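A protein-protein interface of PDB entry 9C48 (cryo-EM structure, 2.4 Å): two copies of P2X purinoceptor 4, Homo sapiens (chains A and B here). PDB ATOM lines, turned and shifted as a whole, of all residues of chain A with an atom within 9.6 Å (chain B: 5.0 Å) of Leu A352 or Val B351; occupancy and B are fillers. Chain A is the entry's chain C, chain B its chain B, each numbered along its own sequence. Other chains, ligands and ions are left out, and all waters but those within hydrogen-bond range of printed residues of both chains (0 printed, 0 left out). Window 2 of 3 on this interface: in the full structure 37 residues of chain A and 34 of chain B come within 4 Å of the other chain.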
ATOM      1  N   ASN A  32      14.668  -2.439  -2.514  1.00  0.00           N
ATOM      2  CA  ASN A  32      15.246  -2.530  -1.188  1.00  0.00           C
ATOM      3  C   ASN A  32      14.358  -3.422  -0.352  1.00  0.00           C
ATOM      4  O   ASN A  32      14.833  -4.351   0.300  1.00  0.00           O
ATOM      5  CB  ASN A  32      15.337  -1.150  -0.554  1.00  0.00           C
ATOM      6  CG  ASN A  32      15.967  -0.126  -1.478  1.00  0.00           C
ATOM      7  OD1 ASN A  32      16.455  -0.462  -2.557  1.00  0.00           O
ATOM      8  ND2 ASN A  32      15.962   1.132  -1.054  1.00  0.00           N
ATOM      9  N   VAL A  35      14.955  -7.004  -1.028  1.00  0.00           N
ATOM     10  CA  VAL A  35      16.208  -7.516  -0.494  1.00  0.00           C
ATOM     11  C   VAL A  35      16.094  -7.744   1.003  1.00  0.00           C
ATOM     12  O   VAL A  35      16.512  -8.785   1.517  1.00  0.00           O
ATOM     13  CB  VAL A  35      17.371  -6.552  -0.764  1.00  0.00           C
ATOM     14  CG1 VAL A  35      18.640  -7.050  -0.092  1.00  0.00           C
ATOM     15  CG2 VAL A  35      17.579  -6.383  -2.259  1.00  0.00           C
ATOM     16  N   ALA A 344      20.786  -6.450  12.338  1.00  0.00           N
ATOM     17  CA  ALA A 344      21.956  -5.730  11.895  1.00  0.00           C
ATOM     18  C   ALA A 344      22.239  -6.122  10.477  1.00  0.00           C
ATOM     19  O   ALA A 344      22.388  -5.266   9.606  1.00  0.00           O
ATOM     20  CB  ALA A 344      23.136  -6.069  12.779  1.00  0.00           C
ATOM     21  N   LEU A 345      22.301  -7.423  10.233  1.00  0.00           N
ATOM     22  CA  LEU A 345      22.617  -7.890   8.905  1.00  0.00           C
ATOM     23  C   LEU A 345      21.680  -7.250   7.925  1.00  0.00           C
ATOM     24  O   LEU A 345      22.125  -6.670   6.948  1.00  0.00           O
ATOM     25  CB  LEU A 345      22.476  -9.403   8.813  1.00  0.00           C
ATOM     26  CG  LEU A 345      22.420  -9.953   7.388  1.00  0.00           C
ATOM     27  CD1 LEU A 345      23.716  -9.656   6.650  1.00  0.00           C
ATOM     28  CD2 LEU A 345      22.126 -11.444   7.391  1.00  0.00           C
ATOM     29  N   LEU A 346      20.386  -7.311   8.193  1.00  0.00           N
ATOM     30  CA  LEU A 346      19.428  -6.798   7.225  1.00  0.00           C
ATOM     31  C   LEU A 346      19.729  -5.356   6.884  1.00  0.00           C
ATOM     32  O   LEU A 346      19.901  -5.013   5.714  1.00  0.00           O
ATOM     33  CB  LEU A 346      18.002  -6.924   7.766  1.00  0.00           C
ATOM     34  CG  LEU A 346      16.847  -6.559   6.830  1.00  0.00           C
ATOM     35  CD1 LEU A 346      15.562  -7.218   7.296  1.00  0.00           C
ATOM     36  CD2 LEU A 346      16.662  -5.054   6.706  1.00  0.00           C
ATOM     37  N   GLY A 347      19.817  -4.509   7.897  1.00  0.00           N
ATOM     38  CA  GLY A 347      20.047  -3.103   7.641  1.00  0.00           C
ATOM     39  C   GLY A 347      21.313  -2.899   6.840  1.00  0.00           C
ATOM     40  O   GLY A 347      21.296  -2.213   5.826  1.00  0.00           O
ATOM     41  N   MET A 348      22.409  -3.515   7.268  1.00  0.00           N
ATOM     42  CA  MET A 348      23.675  -3.306   6.587  1.00  0.00           C
ATOM     43  C   MET A 348      23.553  -3.674   5.123  1.00  0.00           C
ATOM     44  O   MET A 348      23.971  -2.919   4.244  1.00  0.00           O
ATOM     45  CB  MET A 348      24.769  -4.141   7.243  1.00  0.00           C
ATOM     46  CG  MET A 348      25.116  -3.701   8.655  1.00  0.00           C
ATOM     47  SD  MET A 348      26.473  -4.676   9.331  1.00  0.00           S
ATOM     48  CE  MET A 348      25.617  -6.202   9.717  1.00  0.00           C
ATOM     49  N   ALA A 349      22.960  -4.825   4.853  1.00  0.00           N
ATOM     50  CA  ALA A 349      22.813  -5.277   3.483  1.00  0.00           C
ATOM     51  C   ALA A 349      21.959  -4.314   2.685  1.00  0.00           C
ATOM     52  O   ALA A 349      22.358  -3.850   1.608  1.00  0.00           O
ATOM     53  CB  ALA A 349      22.202  -6.665   3.457  1.00  0.00           C
ATOM     54  N   THR A 350      20.779  -4.000   3.204  1.00  0.00           N
ATOM     55  CA  THR A 350      19.882  -3.148   2.444  1.00  0.00           C
ATOM     56  C   THR A 350      20.569  -1.839   2.102  1.00  0.00           C
ATOM     57  O   THR A 350      20.533  -1.388   0.959  1.00  0.00           O
ATOM     58  CB  THR A 350      18.594  -2.845   3.224  1.00  0.00           C
ATOM     59  OG1 THR A 350      17.947  -4.073   3.580  1.00  0.00           O
ATOM     60  CG2 THR A 350      17.650  -2.003   2.381  1.00  0.00           C
ATOM     61  N   VAL A 351      21.245  -1.259   3.099  1.00  0.00           N
ATOM     62  CA  VAL A 351      21.959   0.038   2.896  1.00  0.00           C
ATOM     63  C   VAL A 351      23.145  -0.175   1.953  1.00  0.00           C
ATOM     64  O   VAL A 351      23.412   0.724   1.137  1.00  0.00           O
ATOM     65  CB  VAL A 351      22.404   0.638   4.244  1.00  0.00           C
ATOM     66  CG1 VAL A 351      23.480   1.698   4.073  1.00  0.00           C
ATOM     67  CG2 VAL A 351      21.227   1.184   5.038  1.00  0.00           C
ATOM     68  N   LEU A 352      23.833  -1.315   2.060  1.00  0.00           N
ATOM     69  CA  LEU A 352      24.934  -1.608   1.106  1.00  0.00           C
ATOM     70  C   LEU A 352      24.349  -1.609  -0.308  1.00  0.00           C
ATOM     71  O   LEU A 352      24.942  -0.964  -1.193  1.00  0.00           O
ATOM     72  CB  LEU A 352      25.550  -2.968   1.434  1.00  0.00           C
ATOM     73  CG  LEU A 352      26.632  -2.958   2.512  1.00  0.00           C
ATOM     74  CD1 LEU A 352      27.525  -4.182   2.385  1.00  0.00           C
ATOM     75  CD2 LEU A 352      27.456  -1.683   2.438  1.00  0.00           C
ATOM     76  N   CYS A 353      23.214  -2.286  -0.494  1.00  0.00           N
ATOM     77  CA  CYS A 353      22.565  -2.349  -1.830  1.00  0.00           C
ATOM     78  C   CYS A 353      22.221  -0.931  -2.291  1.00  0.00           C
ATOM     79  O   CYS A 353      22.456  -0.634  -3.467  1.00  0.00           O
ATOM     80  CB  CYS A 353      21.292  -3.185  -1.776  1.00  0.00           C
ATOM     81  SG  CYS A 353      21.574  -4.883  -1.214  1.00  0.00           S
ATOM     82  N   ASP A 354      21.682  -0.100  -1.395  1.00  0.00           N
ATOM     83  CA  ASP A 354      21.315   1.298  -1.746  1.00  0.00           C
ATOM     84  C   ASP A 354      22.561   2.037  -2.245  1.00  0.00           C
ATOM     85  O   ASP A 354      22.487   2.666  -3.323  1.00  0.00           O
ATOM     86  CB  ASP A 354      20.680   2.012  -0.553  1.00  0.00           C
ATOM     87  CG  ASP A 354      19.397   1.349  -0.078  1.00  0.00           C
ATOM     88  OD1 ASP A 354      18.990   0.353  -0.705  1.00  0.00           O
ATOM     89  OD2 ASP A 354      18.826   1.828   0.922  1.00  0.00           O
ATOM     90  N   ILE A 355      23.666   1.934  -1.503  1.00  0.00           N
ATOM     91  CA  ILE A 355      24.938   2.598  -1.917  1.00  0.00           C
ATOM     92  C   ILE A 355      25.318   2.089  -3.309  1.00  0.00           C
ATOM     93  O   ILE A 355      25.566   2.929  -4.184  1.00  0.00           O
ATOM     94  CB  ILE A 355      26.057   2.323  -0.894  1.00  0.00           C
ATOM     95  CG1 ILE A 355      25.710   2.878   0.489  1.00  0.00           C
ATOM     96  CG2 ILE A 355      27.389   2.859  -1.395  1.00  0.00           C
ATOM     97  CD1 ILE A 355      25.481   4.372   0.511  1.00  0.00           C
ATOM     98  N   ILE A 356      25.356   0.768  -3.496  1.00  0.00           N
ATOM     99  CA  ILE A 356      25.780   0.186  -4.805  1.00  0.00           C
ATOM    100  C   ILE A 356      24.876   0.722  -5.921  1.00  0.00           C
ATOM    101  O   ILE A 356      25.408   1.052  -6.997  1.00  0.00           O
ATOM    102  CB  ILE A 356      25.758  -1.354  -4.744  1.00  0.00           C
ATOM    103  CG1 ILE A 356      26.697  -1.888  -3.657  1.00  0.00           C
ATOM    104  CG2 ILE A 356      26.074  -1.957  -6.103  1.00  0.00           C
ATOM    105  CD1 ILE A 356      26.603  -3.379  -3.445  1.00  0.00           C
ATOM    106  N   VAL A 357      23.567   0.811  -5.673  1.00  0.00           N
ATOM    107  CA  VAL A 357      22.611   1.246  -6.738  1.00  0.00           C
ATOM    108  C   VAL A 357      22.981   2.655  -7.212  1.00  0.00           C
ATOM    109  O   VAL A 357      23.041   2.868  -8.438  1.00  0.00           O
ATOM    110  CB  VAL A 357      21.153   1.185  -6.240  1.00  0.00           C
ATOM    111  CG1 VAL A 357      20.213   1.977  -7.135  1.00  0.00           C
ATOM    112  CG2 VAL A 357      20.669  -0.248  -6.089  1.00  0.00           C
ATOM    113  N   LEU A 358      23.225   3.576  -6.276  1.00  0.00           N
ATOM    114  CA  LEU A 358      23.547   4.981  -6.644  1.00  0.00           C
ATOM    115  C   LEU A 358      24.841   5.002  -7.464  1.00  0.00           C
ATOM    116  O   LEU A 358      24.904   5.765  -8.447  1.00  0.00           O
ATOM    117  CB  LEU A 358      23.696   5.806  -5.364  1.00  0.00           C
ATOM    118  CG  LEU A 358      22.478   5.806  -4.441  1.00  0.00           C
ATOM    119  CD1 LEU A 358      22.650   6.819  -3.320  1.00  0.00           C
ATOM    120  CD2 LEU A 358      21.205   6.087  -5.224  1.00  0.00           C
ATOM    121  N   TYR A 359      25.831   4.201  -7.064  1.00  0.00           N
ATOM    122  CA  TYR A 359      27.129   4.154  -7.788  1.00  0.00           C
ATOM    123  C   TYR A 359      26.899   3.649  -9.215  1.00  0.00           C
ATOM    124  O   TYR A 359      27.481   4.222 -10.154  1.00  0.00           O
ATOM    125  CB  TYR A 359      28.131   3.280  -7.029  1.00  0.00           C
ATOM    126  CG  TYR A 359      28.818   3.965  -5.874  1.00  0.00           C
ATOM    127  CD1 TYR A 359      28.089   4.548  -4.851  1.00  0.00           C
ATOM    128  CD2 TYR A 359      30.199   4.046  -5.811  1.00  0.00           C
ATOM    129  CE1 TYR A 359      28.712   5.182  -3.789  1.00  0.00           C
ATOM    130  CE2 TYR A 359      30.839   4.676  -4.756  1.00  0.00           C
ATOM    131  CZ  TYR A 359      30.093   5.247  -3.740  1.00  0.00           C
ATOM    132  OH  TYR A 359      30.720   5.875  -2.692  1.00  0.00           O
ATOM    133  N   CYS A 360      26.069   2.613  -9.369  1.00  0.00           N
ATOM    134  CA  CYS A 360      25.753   2.077 -10.719  1.00  0.00           C
ATOM    135  C   CYS A 360      25.066   3.170 -11.544  1.00  0.00           C
ATOM    136  O   CYS A 360      25.395   3.300 -12.738  1.00  0.00           O
ATOM    137  CB  CYS A 360      24.839   0.863 -10.623  1.00  0.00           C
ATOM    138  SG  CYS A 360      24.389   0.171 -12.236  1.00  0.00           S
ATOM    139  N   ALA B 344      30.597  -8.922   1.772  1.00  0.00           N
ATOM    140  CA  ALA B 344      29.877  -8.065   2.684  1.00  0.00           C
ATOM    141  C   ALA B 344      30.870  -7.191   3.388  1.00  0.00           C
ATOM    142  O   ALA B 344      30.722  -5.970   3.415  1.00  0.00           O
ATOM    143  CB  ALA B 344      29.114  -8.904   3.686  1.00  0.00           C
ATOM    144  N   LEU B 346      33.798  -6.252   2.610  1.00  0.00           N
ATOM    145  CA  LEU B 346      34.398  -5.228   1.768  1.00  0.00           C
ATOM    146  C   LEU B 346      33.468  -4.045   1.616  1.00  0.00           C
ATOM    147  O   LEU B 346      33.848  -2.910   1.908  1.00  0.00           O
ATOM    148  CB  LEU B 346      34.750  -5.802   0.394  1.00  0.00           C
ATOM    149  CG  LEU B 346      35.516  -4.904  -0.583  1.00  0.00           C
ATOM    150  CD1 LEU B 346      36.226  -5.747  -1.627  1.00  0.00           C
ATOM    151  CD2 LEU B 346      34.612  -3.877  -1.248  1.00  0.00           C
ATOM    152  N   GLY B 347      32.245  -4.300   1.180  1.00  0.00           N
ATOM    153  CA  GLY B 347      31.320  -3.210   0.956  1.00  0.00           C
ATOM    154  C   GLY B 347      31.132  -2.393   2.214  1.00  0.00           C
ATOM    155  O   GLY B 347      31.255  -1.174   2.180  1.00  0.00           O
ATOM    156  N   MET B 348      30.865  -3.053   3.334  1.00  0.00           N
ATOM    157  CA  MET B 348      30.604  -2.326   4.565  1.00  0.00           C
ATOM    158  C   MET B 348      31.771  -1.422   4.900  1.00  0.00           C
ATOM    159  O   MET B 348      31.590  -0.243   5.211  1.00  0.00           O
ATOM    160  CB  MET B 348      30.356  -3.302   5.709  1.00  0.00           C
ATOM    161  CG  MET B 348      29.078  -4.109   5.566  1.00  0.00           C
ATOM    162  SD  MET B 348      28.808  -5.173   6.994  1.00  0.00           S
ATOM    163  CE  MET B 348      29.997  -6.473   6.661  1.00  0.00           C
ATOM    164  N   ALA B 349      32.977  -1.962   4.819  1.00  0.00           N
ATOM    165  CA  ALA B 349      34.157  -1.185   5.140  1.00  0.00           C
ATOM    166  C   ALA B 349      34.301  -0.006   4.201  1.00  0.00           C
ATOM    167  O   ALA B 349      34.448   1.145   4.638  1.00  0.00           O
ATOM    168  CB  ALA B 349      35.391  -2.064   5.072  1.00  0.00           C
ATOM    169  N   THR B 350      34.258  -0.276   2.903  1.00  0.00           N
ATOM    170  CA  THR B 350      34.474   0.802   1.955  1.00  0.00           C
ATOM    171  C   THR B 350      33.480   1.921   2.200  1.00  0.00           C
ATOM    172  O   THR B 350      33.852   3.092   2.260  1.00  0.00           O
ATOM    173  CB  THR B 350      34.328   0.317   0.505  1.00  0.00           C
ATOM    174  OG1 THR B 350      35.241  -0.762   0.264  1.00  0.00           O
ATOM    175  CG2 THR B 350      34.620   1.450  -0.466  1.00  0.00           C
ATOM    176  N   VAL B 351      32.213   1.544   2.397  1.00  0.00           N
ATOM    177  CA  VAL B 351      31.136   2.549   2.640  1.00  0.00           C
ATOM    178  C   VAL B 351      31.356   3.212   4.001  1.00  0.00           C
ATOM    179  O   VAL B 351      31.099   4.424   4.110  1.00  0.00           O
ATOM    180  CB  VAL B 351      29.742   1.897   2.545  1.00  0.00           C
ATOM    181  CG1 VAL B 351      28.663   2.748   3.194  1.00  0.00           C
ATOM    182  CG2 VAL B 351      29.374   1.558   1.108  1.00  0.00           C
ATOM    183  N   LEU B 352      31.810   2.452   5.002  1.00  0.00           N
ATOM    184  CA  LEU B 352      32.126   3.071   6.316  1.00  0.00           C
ATOM    185  C   LEU B 352      33.196   4.141   6.092  1.00  0.00           C
ATOM    186  O   LEU B 352      33.025   5.264   6.601  1.00  0.00           O
ATOM    187  CB  LEU B 352      32.633   1.996   7.280  1.00  0.00           C
ATOM    188  CG  LEU B 352      31.553   1.220   8.028  1.00  0.00           C
ATOM    189  CD1 LEU B 352      32.118   0.601   9.296  1.00  0.00           C
ATOM    190  CD2 LEU B 352      30.370   2.117   8.352  1.00  0.00           C
ATOM    191  N   CYS B 353      34.241   3.804   5.331  1.00  0.00           N
ATOM    192  CA  CYS B 353      35.336   4.770   5.053  1.00  0.00           C
ATOM    193  C   CYS B 353      34.757   5.998   4.347  1.00  0.00           C
ATOM    194  O   CYS B 353      35.143   7.112   4.714  1.00  0.00           O
ATOM    195  CB  CYS B 353      36.406   4.139   4.172  1.00  0.00           C
ATOM    196  SG  CYS B 353      37.148   2.655   4.898  1.00  0.00           S
ATOM    197  N   ASP B 354      33.867   5.792   3.371  1.00  0.00           N
ATOM    198  CA  ASP B 354      33.246   6.919   2.627  1.00  0.00           C
ATOM    199  C   ASP B 354      32.516   7.835   3.614  1.00  0.00           C
ATOM    200  O   ASP B 354      32.739   9.063   3.562  1.00  0.00           O
ATOM    201  CB  ASP B 354      32.304   6.402   1.538  1.00  0.00           C
ATOM    202  CG  ASP B 354      33.010   5.550   0.497  1.00  0.00           C
ATOM    203  OD1 ASP B 354      34.242   5.396   0.608  1.00  0.00           O
ATOM    204  OD2 ASP B 354      32.321   5.041  -0.409  1.00  0.00           O
ATOM    205  N   ILE B 355      31.701   7.250   4.496  1.00  0.00           N
ATOM    206  CA  ILE B 355      30.963   8.053   5.515  1.00  0.00           C
ATOM    207  C   ILE B 355      31.982   8.840   6.342  1.00  0.00           C
ATOM    208  O   ILE B 355      31.808  10.059   6.467  1.00  0.00           O
ATOM    209  CB  ILE B 355      30.098   7.143   6.408  1.00  0.00           C
ATOM    210  CG1 ILE B 355      29.038   6.394   5.597  1.00  0.00           C
ATOM    211  CG2 ILE B 355      29.474   7.938   7.545  1.00  0.00           C
ATOM    212  CD1 ILE B 355      28.075   7.299   4.863  1.00  0.00           C
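The side-chain hydroxyl (OH) of Tyr A359 lies within hydrogen-bond range of the side-chain carboxylate (OD2) of Asp B354 (2.9 Å). The side-chain sulfur (SD) of Met B348 sits close to the side-chain sulfur (SD) of Met A348, at 3.3 Å.
Leu A352 touches Ala B344. Leu A352 touches Gly B347 (CD2 to C, 3.8 Å). Leu A352 touches Met B348 (CD1 to CG, 3.5 Å). CD2 of Leu A352 touches CG2 of Val B351, 3.99 Å away. Ile A355 touches Val B351 (CG2 to CG2, 3.4 Å).
Asn A32 touches none of the printed residues of chain B. Of the printed residues of chain B, Met A348 touches Met B348. Printed residues of chain B within 4 Å of Leu A352: Ala B344, Gly B347, Met B348 and Val B351. Asp A354 touches none of the printed residues of chain B. Of the printed residues of chain B, Ile A355 touches Val B351. Of the printed residues of chain B, Tyr A359 touches Asp B354. Printed residues of chain A within 4 Å of Ala B344: Leu A352 (3.8 Å). Gly B347 touches one residue of chain A. Met B348 touches just these residues of chain A: Met A348 and Leu A352. No residue of chain A comes within 4 Å of Ala B349. Of the printed residues of chain A, Val B351 touches Leu A352 and Ile A355. Of chain A, only Tyr A359 (2.9 Å) comes within 4 Å of Asp B354. The nearest printed residue of chain B that does not touch Leu A352 is Leu B346 (6.0 Å). The nearest printed residue of chain B that does not touch Met A348 is Ala B344 (7.3 Å).
Hydrophobic or aromatic side chains of chain B that line the printed part of chain A: Met B348 and Val B351. Among the printed residues, no Asp or Glu carboxylate lies within 4 Å of a Lys or Arg side-chain nitrogen of the other chain.
Leu A352 touches Ala B344, but with the chains exchanged Ala A344 does not touch Leu B352 (10.9 Å). Leu A352 touches Gly B347, but with the chains exchanged Gly A347 does not touch Leu B352 (10.4 Å). Leu A352 touches Met B348, but with the chains exchanged Met A348 does not touch Leu B352 (7.7 Å). Ile A355 touches Val B351, but with the chains exchanged Val A351 does not touch Ile B355 (7.3 Å). Of the 7 pairs that touch across the chains among the printed residues, 1 has its exchanged pair printed and touching as well.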
